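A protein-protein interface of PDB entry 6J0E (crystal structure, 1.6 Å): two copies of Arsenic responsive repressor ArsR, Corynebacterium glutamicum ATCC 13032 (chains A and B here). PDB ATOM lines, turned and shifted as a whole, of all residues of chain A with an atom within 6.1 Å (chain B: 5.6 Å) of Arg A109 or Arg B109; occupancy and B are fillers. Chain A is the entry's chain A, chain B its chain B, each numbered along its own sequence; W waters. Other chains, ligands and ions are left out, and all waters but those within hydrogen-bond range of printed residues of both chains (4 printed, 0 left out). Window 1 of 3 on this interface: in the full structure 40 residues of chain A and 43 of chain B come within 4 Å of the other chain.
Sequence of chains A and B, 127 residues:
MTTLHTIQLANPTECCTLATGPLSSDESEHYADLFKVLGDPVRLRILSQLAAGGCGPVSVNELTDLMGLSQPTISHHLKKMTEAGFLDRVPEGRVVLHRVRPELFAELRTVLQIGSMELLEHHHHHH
Among the printed residues, merely in contact across the chains: Arg A109 with Arg B109 (3.3 Å), Phe A105 with Leu B112 (3.5 Å), Met A117 with Arg B109 (3.5 Å), Arg A109 with Met B117 (3.6 Å), Pro A102 with Ile B114 (3.6 Å), Leu A112 with Phe B105 (3.6 Å), Phe A105 with Ile B114 (3.7 Å), Leu A108 with Leu B112 (3.8 Å), Ala A106 with Ser B116 (3.8 Å), Arg A109 with Thr B6 (3.8 Å), Arg A109 with Gln B113 (3.8 Å), Ile A114 with Arg B109 (3.8 Å), Leu A112 with Leu B108 (3.9 Å), Gln A113 with Arg B109 (3.9 Å), Arg A109 with Ile B114 (3.97 Å) and Leu A112 with Leu B112 (3.99 Å).
OG1 of Thr A110 lies within hydrogen-bond range of O of Ala A106, 3.1 Å away.
The side-chain hydroxyl (OG1) of Thr B6 is in hydrogen-bond range of the side-chain carboxylate (OE2) of Glu B118, 2.5 Å away.
The backbone carbonyl oxygen (O) of Ser B116 is in hydrogen-bond range of the side-chain amide nitrogen (NE2) of Gln B113.
Water W2 lies within hydrogen-bond range of the backbone carbonyl oxygen (O) of Ile A114 (2.5 Å), the backbone carbonyl oxygen (O) of Pro B102 (2.7 Å), the guanidinium group (NH1) of Arg B109 (2.9 Å) and the backbone NH (N) of Ala B106 (3.5 Å).
Water W3 bridges the guanidinium group of Arg B109 (2.5 Å) and the backbone carbonyl oxygen of Ser A116 (2.8 Å).
Water W1 lies within hydrogen-bond range of the side-chain hydroxyl (OG) of Ser B116 (2.6 Å), the backbone carbonyl oxygen (O) of Pro A102 (2.7 Å), the backbone carbonyl oxygen (O) of Ile B114 (2.8 Å) and the guanidinium group (NH1) of Arg A109 (2.9 Å).
Water W4 lies within hydrogen-bond range of the side-chain carboxylate (OE1) of Glu B118 (2.7 Å) and the side-chain amide nitrogen (NE2) of Gln A113 (3.0 Å).
Of the printed residues of chain B, Arg A109 touches Thr B6 (3.8 Å), Arg B109 (3.3 Å), Leu B112 (2.8 Å), Gln B113 (3.8 Å), Ile B114 (3.97 Å), Ser B116 (2.8 Å), Met B117 (3.6 Å) and Glu B118 (2.7 Å).
Of chain A, only Arg A109, Leu A112, Gln A113, Ile A114 and Met A117 come within 4 Å of Arg B109.
Of the printed residues of chain A, Gln B113 touches Arg A109 (3.8 Å).
Printed residues of chain B within 4 Å of Gln A113: Arg B109 (3.9 Å).
Of the printed residues of chain B, Ala A106 touches Ser B116.
Printed residues of chain B within 4 Å of Phe A105: Leu B112 (3.5 Å) and Ile B114 (3.7 Å).
Thr B110 touches none of the printed residues of chain A.
The nearest printed residue of chain A that does not touch Leu B112 is Ala A106 (5.0 Å).
Of the 16 printed residues of chain B, 10 touch a printed residue of chain A.
Hydrophobic or aromatic side chains of chain B that line the printed part of chain A: Phe B105, Leu B108, Leu B112 and Ile B114.
Along chain B the printed residues that touch a printed residue of chain A span positions 6 to 118.
Hydrophobic or aromatic side chains of chain A within 4 Å of the printed part of chain B: Pro A102, Phe A105, Ala A106, Leu A108, Leu A112 and Met A117.
Along chain A the printed residues that touch a printed residue of chain B span positions 102 to 117.
Among the printed residues, Asp or Glu carboxylates within 4 Å of a Lys or Arg side-chain nitrogen of the other chain: Arg A109 with Glu B118 (2.7 Å).
Pro A102 touches Ile B114, but with the chains exchanged Ile A114 does not touch Pro B102 (4.05 Å).
Phe A105 touches Leu B112, and with the chains exchanged Leu A112 touches Phe B105.
Arg A109 touches Ser B116, but with the chains exchanged Ser A116 does not touch Arg B109 (4.9 Å).
Arg A109 touches Glu B118, but with the chains exchanged Glu A118 does not touch Arg B109 (5.7 Å).
The backbone carbonyl oxygen (O) of Leu B112 lies within hydrogen-bond range of the guanidinium group (NH1) of Arg A109.
OG of Ser B116 is in hydrogen-bond range of NH2 of Arg A109.
The guanidinium group of Arg A109 lies within salt-bridge range of the side-chain carboxylate of Glu B118.
The backbone carbonyl oxygen of Leu A112 sits at hydrogen-bond distance from the guanidinium group of Arg B109 (3.0 Å).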
ATOM      1  N   PRO A 102      -3.864  -9.495 -21.117  1.00  0.00           N
ATOM      2  CA  PRO A 102      -2.957 -10.572 -21.389  1.00  0.00           C
ATOM      3  C   PRO A 102      -3.523 -11.939 -21.277  1.00  0.00           C
ATOM      4  O   PRO A 102      -2.950 -12.944 -21.881  1.00  0.00           O
ATOM      5  CB  PRO A 102      -1.897 -10.369 -20.332  1.00  0.00           C
ATOM      6  CG  PRO A 102      -2.629  -9.759 -19.172  1.00  0.00           C
ATOM      7  CD  PRO A 102      -3.511  -8.805 -19.855  1.00  0.00           C
ATOM      8  N   LEU A 104      -6.163 -14.061 -22.303  1.00  0.00           N
ATOM      9  CA  LEU A 104      -6.497 -15.034 -23.305  1.00  0.00           C
ATOM     10  C   LEU A 104      -5.285 -15.406 -24.174  1.00  0.00           C
ATOM     11  O   LEU A 104      -5.232 -16.570 -24.607  1.00  0.00           O
ATOM     12  CB  LEU A 104      -7.727 -14.712 -24.192  1.00  0.00           C
ATOM     13  CG  LEU A 104      -9.026 -14.546 -23.374  1.00  0.00           C
ATOM     14  CD1 LEU A 104     -10.225 -14.103 -24.215  1.00  0.00           C
ATOM     15  CD2 LEU A 104      -9.358 -15.828 -22.664  1.00  0.00           C
ATOM     16  N   PHE A 105      -4.396 -14.443 -24.356  1.00  0.00           N
ATOM     17  CA  PHE A 105      -3.143 -14.710 -25.159  1.00  0.00           C
ATOM     18  C   PHE A 105      -2.397 -15.820 -24.426  1.00  0.00           C
ATOM     19  O   PHE A 105      -1.873 -16.717 -25.053  1.00  0.00           O
ATOM     20  CB  PHE A 105      -2.314 -13.472 -25.354  1.00  0.00           C
ATOM     21  CG  PHE A 105      -3.004 -12.392 -26.132  1.00  0.00           C
ATOM     22  CD1 PHE A 105      -3.100 -12.581 -27.489  1.00  0.00           C
ATOM     23  CD2 PHE A 105      -3.453 -11.222 -25.542  1.00  0.00           C
ATOM     24  CE1 PHE A 105      -3.772 -11.634 -28.263  1.00  0.00           C
ATOM     25  CE2 PHE A 105      -4.112 -10.265 -26.305  1.00  0.00           C
ATOM     26  CZ  PHE A 105      -4.272 -10.493 -27.648  1.00  0.00           C
ATOM     27  N   ALA A 106      -2.297 -15.721 -23.086  1.00  0.00           N
ATOM     28  CA  ALA A 106      -1.603 -16.840 -22.385  1.00  0.00           C
ATOM     29  C   ALA A 106      -2.289 -18.174 -22.484  1.00  0.00           C
ATOM     30  O   ALA A 106      -1.647 -19.223 -22.644  1.00  0.00           O
ATOM     31  CB  ALA A 106      -1.458 -16.362 -20.906  1.00  0.00           C
ATOM     32  N   GLU A 107      -3.640 -18.224 -22.462  1.00  0.00           N
ATOM     33  CA  GLU A 107      -4.327 -19.475 -22.629  1.00  0.00           C
ATOM     34  C   GLU A 107      -4.039 -20.079 -24.030  1.00  0.00           C
ATOM     35  O   GLU A 107      -3.841 -21.231 -24.220  1.00  0.00           O
ATOM     36  CB  GLU A 107      -5.896 -19.414 -22.465  1.00  0.00           C
ATOM     37  CG  GLU A 107      -6.343 -18.997 -21.130  1.00  0.00           C
ATOM     38  CD  GLU A 107      -7.872 -19.025 -21.029  1.00  0.00           C
ATOM     39  OE1 GLU A 107      -8.608 -19.643 -21.876  1.00  0.00           O
ATOM     40  OE2 GLU A 107      -8.250 -18.427 -20.013  1.00  0.00           O
ATOM     41  N   LEU A 108      -4.025 -19.186 -25.072  1.00  0.00           N
ATOM     42  CA  LEU A 108      -3.719 -19.674 -26.379  1.00  0.00           C
ATOM     43  C   LEU A 108      -2.265 -20.177 -26.570  1.00  0.00           C
ATOM     44  O   LEU A 108      -2.051 -21.135 -27.208  1.00  0.00           O
ATOM     45  CB  LEU A 108      -3.916 -18.477 -27.408  1.00  0.00           C
ATOM     46  CG  LEU A 108      -5.375 -17.997 -27.524  1.00  0.00           C
ATOM     47  CD1 LEU A 108      -5.490 -16.983 -28.577  1.00  0.00           C
ATOM     48  CD2 LEU A 108      -6.292 -19.180 -27.918  1.00  0.00           C
ATOM     49  N   ARG A 109      -1.332 -19.525 -25.873  1.00  0.00           N
ATOM     50  CA  ARG A 109       0.019 -20.034 -25.824  1.00  0.00           C
ATOM     51  C   ARG A 109       0.023 -21.455 -25.213  1.00  0.00           C
ATOM     52  O   ARG A 109       0.681 -22.346 -25.761  1.00  0.00           O
ATOM     53  CB  ARG A 109       0.893 -19.136 -25.085  1.00  0.00           C
ATOM     54  CG  ARG A 109       1.337 -17.831 -25.788  1.00  0.00           C
ATOM     55  CD  ARG A 109       2.480 -17.132 -25.174  1.00  0.00           C
ATOM     56  NE  ARG A 109       2.400 -16.988 -23.689  1.00  0.00           N
ATOM     57  CZ  ARG A 109       1.835 -15.933 -23.058  1.00  0.00           C
ATOM     58  NH1 ARG A 109       1.206 -14.946 -23.780  1.00  0.00           N
ATOM     59  NH2 ARG A 109       1.867 -15.841 -21.676  1.00  0.00           N
ATOM     60  N   THR A 110      -0.683 -21.616 -24.161  1.00  0.00           N
ATOM     61  CA  THR A 110      -0.773 -22.996 -23.585  1.00  0.00           C
ATOM     62  C   THR A 110      -1.320 -23.977 -24.575  1.00  0.00           C
ATOM     63  O   THR A 110      -0.797 -25.083 -24.778  1.00  0.00           O
ATOM     64  CB  THR A 110      -1.580 -22.910 -22.304  1.00  0.00           C
ATOM     65  OG1 THR A 110      -0.997 -21.963 -21.462  1.00  0.00           O
ATOM     66  CG2 THR A 110      -1.747 -24.282 -21.617  1.00  0.00           C
ATOM     67  N   VAL A 111      -2.401 -23.680 -25.248  1.00  0.00           N
ATOM     68  CA  VAL A 111      -2.942 -24.561 -26.228  1.00  0.00           C
ATOM     69  C   VAL A 111      -1.929 -24.918 -27.271  1.00  0.00           C
ATOM     70  O   VAL A 111      -1.962 -26.040 -27.785  1.00  0.00           O
ATOM     71  CB  VAL A 111      -4.187 -23.953 -26.881  1.00  0.00           C
ATOM     72  CG1 VAL A 111      -4.707 -24.822 -28.010  1.00  0.00           C
ATOM     73  CG2 VAL A 111      -5.290 -23.748 -25.830  1.00  0.00           C
ATOM     74  N   LEU A 112      -1.027 -24.019 -27.603  1.00  0.00           N
ATOM     75  CA  LEU A 112      -0.105 -24.245 -28.694  1.00  0.00           C
ATOM     76  C   LEU A 112       1.244 -24.757 -28.141  1.00  0.00           C
ATOM     77  O   LEU A 112       2.212 -24.688 -28.881  1.00  0.00           O
ATOM     78  CB  LEU A 112       0.150 -22.925 -29.423  1.00  0.00           C
ATOM     79  CG  LEU A 112      -1.195 -22.486 -30.101  1.00  0.00           C
ATOM     80  CD1 LEU A 112      -0.829 -21.399 -31.027  1.00  0.00           C
ATOM     81  CD2 LEU A 112      -1.850 -23.621 -30.859  1.00  0.00           C
ATOM     82  N   GLN A 113       1.284 -25.292 -26.946  1.00  0.00           N
ATOM     83  CA  GLN A 113       2.607 -25.748 -26.329  1.00  0.00           C
ATOM     84  C   GLN A 113       2.930 -27.143 -26.889  1.00  0.00           C
ATOM     85  O   GLN A 113       2.997 -28.106 -26.129  1.00  0.00           O
ATOM     86  CB  GLN A 113       2.637 -25.726 -24.761  1.00  0.00           C
ATOM     87  CG  GLN A 113       2.759 -24.323 -24.116  1.00  0.00           C
ATOM     88  CD  GLN A 113       2.526 -24.234 -22.575  1.00  0.00           C
ATOM     89  OE1 GLN A 113       2.114 -25.191 -21.936  1.00  0.00           O
ATOM     90  NE2 GLN A 113       2.777 -23.079 -22.006  1.00  0.00           N
ATOM     91  N   ILE A 114       3.039 -27.267 -28.163  1.00  0.00           N
ATOM     92  CA  ILE A 114       3.268 -28.514 -28.840  1.00  0.00           C
ATOM     93  C   ILE A 114       4.750 -28.600 -29.158  1.00  0.00           C
ATOM     94  O   ILE A 114       5.263 -27.792 -29.826  1.00  0.00           O
ATOM     95  CB  ILE A 114       2.292 -28.653 -30.059  1.00  0.00           C
ATOM     96  CG1 ILE A 114       0.852 -28.864 -29.517  1.00  0.00           C
ATOM     97  CG2 ILE A 114       2.594 -29.841 -30.884  1.00  0.00           C
ATOM     98  CD1 ILE A 114      -0.178 -28.565 -30.577  1.00  0.00           C
ATOM     99  N   GLY A 115       5.488 -29.582 -28.650  1.00  0.00           N
ATOM    100  CA  GLY A 115       6.878 -29.709 -28.948  1.00  0.00           C
ATOM    101  C   GLY A 115       7.649 -29.447 -27.701  1.00  0.00           C
ATOM    102  O   GLY A 115       7.044 -29.207 -26.690  1.00  0.00           O
ATOM    103  N   SER A 116       8.960 -29.670 -27.764  1.00  0.00           N
ATOM    104  CA  SER A 116       9.844 -29.374 -26.623  1.00  0.00           C
ATOM    105  C   SER A 116       9.975 -27.882 -26.567  1.00  0.00           C
ATOM    106  O   SER A 116      10.293 -27.286 -27.585  1.00  0.00           O
ATOM    107  CB  SER A 116      11.174 -30.061 -26.852  1.00  0.00           C
ATOM    108  OG  SER A 116      12.131 -29.629 -25.903  1.00  0.00           O
ATOM    109  N   MET A 117       9.755 -27.269 -25.408  1.00  0.00           N
ATOM    110  CA  MET A 117      10.032 -25.830 -25.226  1.00  0.00           C
ATOM    111  C   MET A 117      11.361 -25.466 -24.544  1.00  0.00           C
ATOM    112  O   MET A 117      11.838 -26.151 -23.676  1.00  0.00           O
ATOM    113  CB  MET A 117       9.005 -25.223 -24.373  1.00  0.00           C
ATOM    114  CG  MET A 117       7.719 -25.049 -25.104  1.00  0.00           C
ATOM    115  SD  MET A 117       6.463 -24.478 -23.996  1.00  0.00           S
ATOM    116  CE  MET A 117       6.466 -25.550 -22.551  1.00  0.00           C
ATOM    117  N   GLU A 118      11.892 -24.339 -25.004  1.00  0.00           N
ATOM    118  CA  GLU A 118      13.099 -23.741 -24.586  1.00  0.00           C
ATOM    119  C   GLU A 118      12.604 -22.630 -23.684  1.00  0.00           C
ATOM    120  O   GLU A 118      11.949 -21.701 -24.153  1.00  0.00           O
ATOM    121  CB  GLU A 118      13.830 -23.082 -25.799  1.00  0.00           C
ATOM    122  CG  GLU A 118      14.619 -24.041 -26.707  1.00  0.00           C
ATOM    123  CD  GLU A 118      14.643 -23.604 -28.177  1.00  0.00           C
ATOM    124  OE1 GLU A 118      14.824 -24.474 -29.016  1.00  0.00           O
ATOM    125  OE2 GLU A 118      14.466 -22.409 -28.507  1.00  0.00           O
ATOM    126  N   THR B   6       3.401 -18.287 -15.477  1.00  0.00           N
ATOM    127  CA  THR B   6       3.204 -17.162 -16.392  1.00  0.00           C
ATOM    128  C   THR B   6       3.348 -15.890 -15.623  1.00  0.00           C
ATOM    129  O   THR B   6       2.627 -15.687 -14.661  1.00  0.00           O
ATOM    130  CB  THR B   6       1.791 -17.298 -17.063  1.00  0.00           C
ATOM    131  OG1 THR B   6       1.706 -18.442 -17.860  1.00  0.00           O
ATOM    132  CG2 THR B   6       1.486 -15.984 -17.910  1.00  0.00           C
ATOM    133  N   PRO B 102       6.870 -28.905 -34.615  1.00  0.00           N
ATOM    134  CA  PRO B 102       6.990 -27.942 -33.522  1.00  0.00           C
ATOM    135  C   PRO B 102       7.302 -26.516 -33.905  1.00  0.00           C
ATOM    136  O   PRO B 102       6.958 -25.594 -33.147  1.00  0.00           O
ATOM    137  CB  PRO B 102       8.079 -28.484 -32.652  1.00  0.00           C
ATOM    138  CG  PRO B 102       8.602 -29.681 -33.283  1.00  0.00           C
ATOM    139  CD  PRO B 102       7.900 -29.986 -34.538  1.00  0.00           C
ATOM    140  N   LEU B 104       6.307 -24.107 -36.330  1.00  0.00           N
ATOM    141  CA  LEU B 104       5.272 -23.097 -36.436  1.00  0.00           C
ATOM    142  C   LEU B 104       4.648 -22.829 -35.087  1.00  0.00           C
ATOM    143  O   LEU B 104       4.212 -21.747 -34.852  1.00  0.00           O
ATOM    144  CB  LEU B 104       4.138 -23.343 -37.494  1.00  0.00           C
ATOM    145  CG  LEU B 104       4.599 -23.135 -38.935  1.00  0.00           C
ATOM    146  CD1 LEU B 104       3.341 -23.356 -39.747  1.00  0.00           C
ATOM    147  CD2 LEU B 104       5.154 -21.748 -39.197  1.00  0.00           C
ATOM    148  N   PHE B 105       4.543 -23.825 -34.249  1.00  0.00           N
ATOM    149  CA  PHE B 105       3.855 -23.595 -33.005  1.00  0.00           C
ATOM    150  C   PHE B 105       4.690 -22.683 -32.187  1.00  0.00           C
ATOM    151  O   PHE B 105       4.192 -21.849 -31.503  1.00  0.00           O
ATOM    152  CB  PHE B 105       3.498 -24.933 -32.287  1.00  0.00           C
ATOM    153  CG  PHE B 105       2.452 -25.696 -33.012  1.00  0.00           C
ATOM    154  CD1 PHE B 105       1.063 -25.321 -32.939  1.00  0.00           C
ATOM    155  CD2 PHE B 105       2.780 -26.774 -33.864  1.00  0.00           C
ATOM    156  CE1 PHE B 105       0.101 -25.976 -33.679  1.00  0.00           C
ATOM    157  CE2 PHE B 105       1.794 -27.424 -34.544  1.00  0.00           C
ATOM    158  CZ  PHE B 105       0.462 -27.051 -34.496  1.00  0.00           C
ATOM    159  N   ALA B 106       5.988 -22.935 -32.154  1.00  0.00           N
ATOM    160  CA  ALA B 106       6.912 -22.029 -31.410  1.00  0.00           C
ATOM    161  C   ALA B 106       6.855 -20.582 -31.951  1.00  0.00           C
ATOM    162  O   ALA B 106       6.820 -19.621 -31.161  1.00  0.00           O
ATOM    163  CB  ALA B 106       8.329 -22.555 -31.459  1.00  0.00           C
ATOM    164  N   GLU B 107       6.736 -20.424 -33.228  1.00  0.00           N
ATOM    165  CA  GLU B 107       6.610 -19.131 -33.824  1.00  0.00           C
ATOM    166  C   GLU B 107       5.302 -18.459 -33.357  1.00  0.00           C
ATOM    167  O   GLU B 107       5.336 -17.265 -32.998  1.00  0.00           O
ATOM    168  CB  GLU B 107       6.515 -19.179 -35.419  1.00  0.00           C
ATOM    169  CG  GLU B 107       7.854 -19.530 -36.017  1.00  0.00           C
ATOM    170  CD  GLU B 107       7.970 -19.051 -37.489  1.00  0.00           C
ATOM    171  OE1 GLU B 107       6.939 -18.787 -38.161  1.00  0.00           O
ATOM    172  OE2 GLU B 107       9.174 -18.998 -37.966  1.00  0.00           O
ATOM    173  N   LEU B 108       4.192 -19.187 -33.396  1.00  0.00           N
ATOM    174  CA  LEU B 108       2.845 -18.682 -32.961  1.00  0.00           C
ATOM    175  C   LEU B 108       2.881 -18.299 -31.473  1.00  0.00           C
ATOM    176  O   LEU B 108       2.265 -17.312 -31.089  1.00  0.00           O
ATOM    177  CB  LEU B 108       1.660 -19.609 -33.375  1.00  0.00           C
ATOM    178  CG  LEU B 108       1.434 -19.844 -34.826  1.00  0.00           C
ATOM    179  CD1 LEU B 108       0.221 -20.707 -34.984  1.00  0.00           C
ATOM    180  CD2 LEU B 108       1.268 -18.531 -35.610  1.00  0.00           C
ATOM    181  N   ARG B 109       3.517 -19.124 -30.617  1.00  0.00           N
ATOM    182  CA  ARG B 109       3.743 -18.725 -29.214  1.00  0.00           C
ATOM    183  C   ARG B 109       4.401 -17.412 -29.005  1.00  0.00           C
ATOM    184  O   ARG B 109       3.986 -16.680 -28.113  1.00  0.00           O
ATOM    185  CB  ARG B 109       4.443 -19.777 -28.409  1.00  0.00           C
ATOM    186  CG  ARG B 109       3.596 -20.992 -28.208  1.00  0.00           C
ATOM    187  CD  ARG B 109       4.232 -21.973 -27.136  1.00  0.00           C
ATOM    188  NE  ARG B 109       5.609 -22.304 -27.334  1.00  0.00           N
ATOM    189  CZ  ARG B 109       6.030 -23.326 -28.108  1.00  0.00           C
ATOM    190  NH1 ARG B 109       5.117 -24.088 -28.801  1.00  0.00           N
ATOM    191  NH2 ARG B 109       7.281 -23.499 -28.234  1.00  0.00           N
ATOM    192  N   THR B 110       5.404 -17.073 -29.860  1.00  0.00           N
ATOM    193  CA  THR B 110       6.076 -15.802 -29.840  1.00  0.00           C
ATOM    194  C   THR B 110       5.144 -14.653 -30.288  1.00  0.00           C
ATOM    195  O   THR B 110       5.122 -13.556 -29.673  1.00  0.00           O
ATOM    196  CB  THR B 110       7.320 -15.820 -30.734  1.00  0.00           C
ATOM    197  OG1 THR B 110       8.155 -16.890 -30.284  1.00  0.00           O
ATOM    198  CG2 THR B 110       7.982 -14.511 -30.795  1.00  0.00           C
ATOM    199  N   VAL B 111       4.338 -14.885 -31.279  1.00  0.00           N
ATOM    200  CA  VAL B 111       3.447 -13.807 -31.791  1.00  0.00           C
ATOM    201  C   VAL B 111       2.394 -13.422 -30.726  1.00  0.00           C
ATOM    202  O   VAL B 111       1.893 -12.437 -30.644  1.00  0.00           O
ATOM    203  CB  VAL B 111       2.720 -14.325 -33.069  1.00  0.00           C
ATOM    204  CG1 VAL B 111       1.542 -13.528 -33.529  1.00  0.00           C
ATOM    205  CG2 VAL B 111       3.705 -14.428 -34.246  1.00  0.00           C
ATOM    206  N   LEU B 112       2.083 -14.417 -29.885  1.00  0.00           N
ATOM    207  CA  LEU B 112       1.076 -14.306 -28.820  1.00  0.00           C
ATOM    208  C   LEU B 112       1.697 -13.959 -27.423  1.00  0.00           C
ATOM    209  O   LEU B 112       0.946 -14.058 -26.451  1.00  0.00           O
ATOM    210  CB  LEU B 112       0.322 -15.635 -28.663  1.00  0.00           C
ATOM    211  CG  LEU B 112      -0.544 -16.234 -29.816  1.00  0.00           C
ATOM    212  CD1 LEU B 112      -0.877 -17.714 -29.495  1.00  0.00           C
ATOM    213  CD2 LEU B 112      -1.791 -15.521 -29.953  1.00  0.00           C
ATOM    214  N   GLN B 113       2.933 -13.566 -27.367  1.00  0.00           N
ATOM    215  CA  GLN B 113       3.598 -13.194 -26.145  1.00  0.00           C
ATOM    216  C   GLN B 113       3.277 -11.681 -25.919  1.00  0.00           C
ATOM    217  O   GLN B 113       4.058 -10.843 -26.215  1.00  0.00           O
ATOM    218  CB  GLN B 113       5.058 -13.495 -26.280  1.00  0.00           C
ATOM    219  CG  GLN B 113       5.872 -13.209 -24.989  1.00  0.00           C
ATOM    220  CD  GLN B 113       6.122 -11.720 -24.728  1.00  0.00           C
ATOM    221  OE1 GLN B 113       6.884 -10.997 -25.511  1.00  0.00           O
ATOM    222  NE2 GLN B 113       5.531 -11.231 -23.584  1.00  0.00           N
ATOM    223  N   ILE B 114       2.055 -11.445 -25.443  1.00  0.00           N
ATOM    224  CA  ILE B 114       1.451 -10.137 -25.330  1.00  0.00           C
ATOM    225  C   ILE B 114       1.201  -9.807 -23.831  1.00  0.00           C
ATOM    226  O   ILE B 114       0.216 -10.211 -23.266  1.00  0.00           O
ATOM    227  CB  ILE B 114       0.041 -10.157 -26.048  1.00  0.00           C
ATOM    228  CG1 ILE B 114       0.222 -10.614 -27.501  1.00  0.00           C
ATOM    229  CG2 ILE B 114      -0.574  -8.723 -25.970  1.00  0.00           C
ATOM    230  CD1 ILE B 114       0.963  -9.675 -28.307  1.00  0.00           C
ATOM    231  N   SER B 116       2.805 -11.014 -21.164  1.00  0.00           N
ATOM    232  CA  SER B 116       3.088 -12.101 -20.192  1.00  0.00           C
ATOM    233  C   SER B 116       3.856 -13.147 -20.969  1.00  0.00           C
ATOM    234  O   SER B 116       3.883 -13.150 -22.231  1.00  0.00           O
ATOM    235  CB  SER B 116       1.850 -12.667 -19.540  1.00  0.00           C
ATOM    236  OG  SER B 116       0.963 -13.512 -20.330  1.00  0.00           O
ATOM    237  N   MET B 117       4.551 -14.006 -20.227  1.00  0.00           N
ATOM    238  CA  MET B 117       5.364 -15.028 -20.798  1.00  0.00           C
ATOM    239  C   MET B 117       5.496 -16.142 -19.750  1.00  0.00           C
ATOM    240  O   MET B 117       5.310 -15.862 -18.607  1.00  0.00           O
ATOM    241  CB  MET B 117       6.747 -14.514 -21.201  1.00  0.00           C
ATOM    242  CG  MET B 117       7.606 -14.003 -20.092  1.00  0.00           C
ATOM    243  SD  MET B 117       9.271 -13.577 -20.595  1.00  0.00           S
ATOM    244  CE  MET B 117      10.076 -15.105 -21.020  1.00  0.00           C
ATOM    245  N   GLU B 118       5.876 -17.303 -20.240  1.00  0.00           N
ATOM    246  CA  GLU B 118       6.129 -18.530 -19.389  1.00  0.00           C
ATOM    247  C   GLU B 118       7.553 -18.667 -19.178  1.00  0.00           C
ATOM    248  O   GLU B 118       8.317 -18.811 -20.153  1.00  0.00           O
ATOM    249  CB  GLU B 118       5.407 -19.789 -20.041  1.00  0.00           C
ATOM    250  CG  GLU B 118       3.956 -19.818 -19.814  1.00  0.00           C
ATOM    251  CD  GLU B 118       3.193 -18.709 -20.659  1.00  0.00           C
ATOM    252  OE1 GLU B 118       3.698 -18.776 -21.959  1.00  0.00           O
ATOM    253  OE2 GLU B 118       2.473 -17.943 -20.179  1.00  0.00           O
HETATM  254  O   HOH W   1      -0.314 -12.815 -22.480  1.00  0.00           O
HETATM  255  O   HOH W   2       6.666 -25.859 -30.440  1.00  0.00           O
HETATM  256  O   HOH W   3       8.597 -25.516 -29.035  1.00  0.00           O
HETATM  257  O   HOH W   4       4.116 -20.898 -23.613  1.00  0.00           O
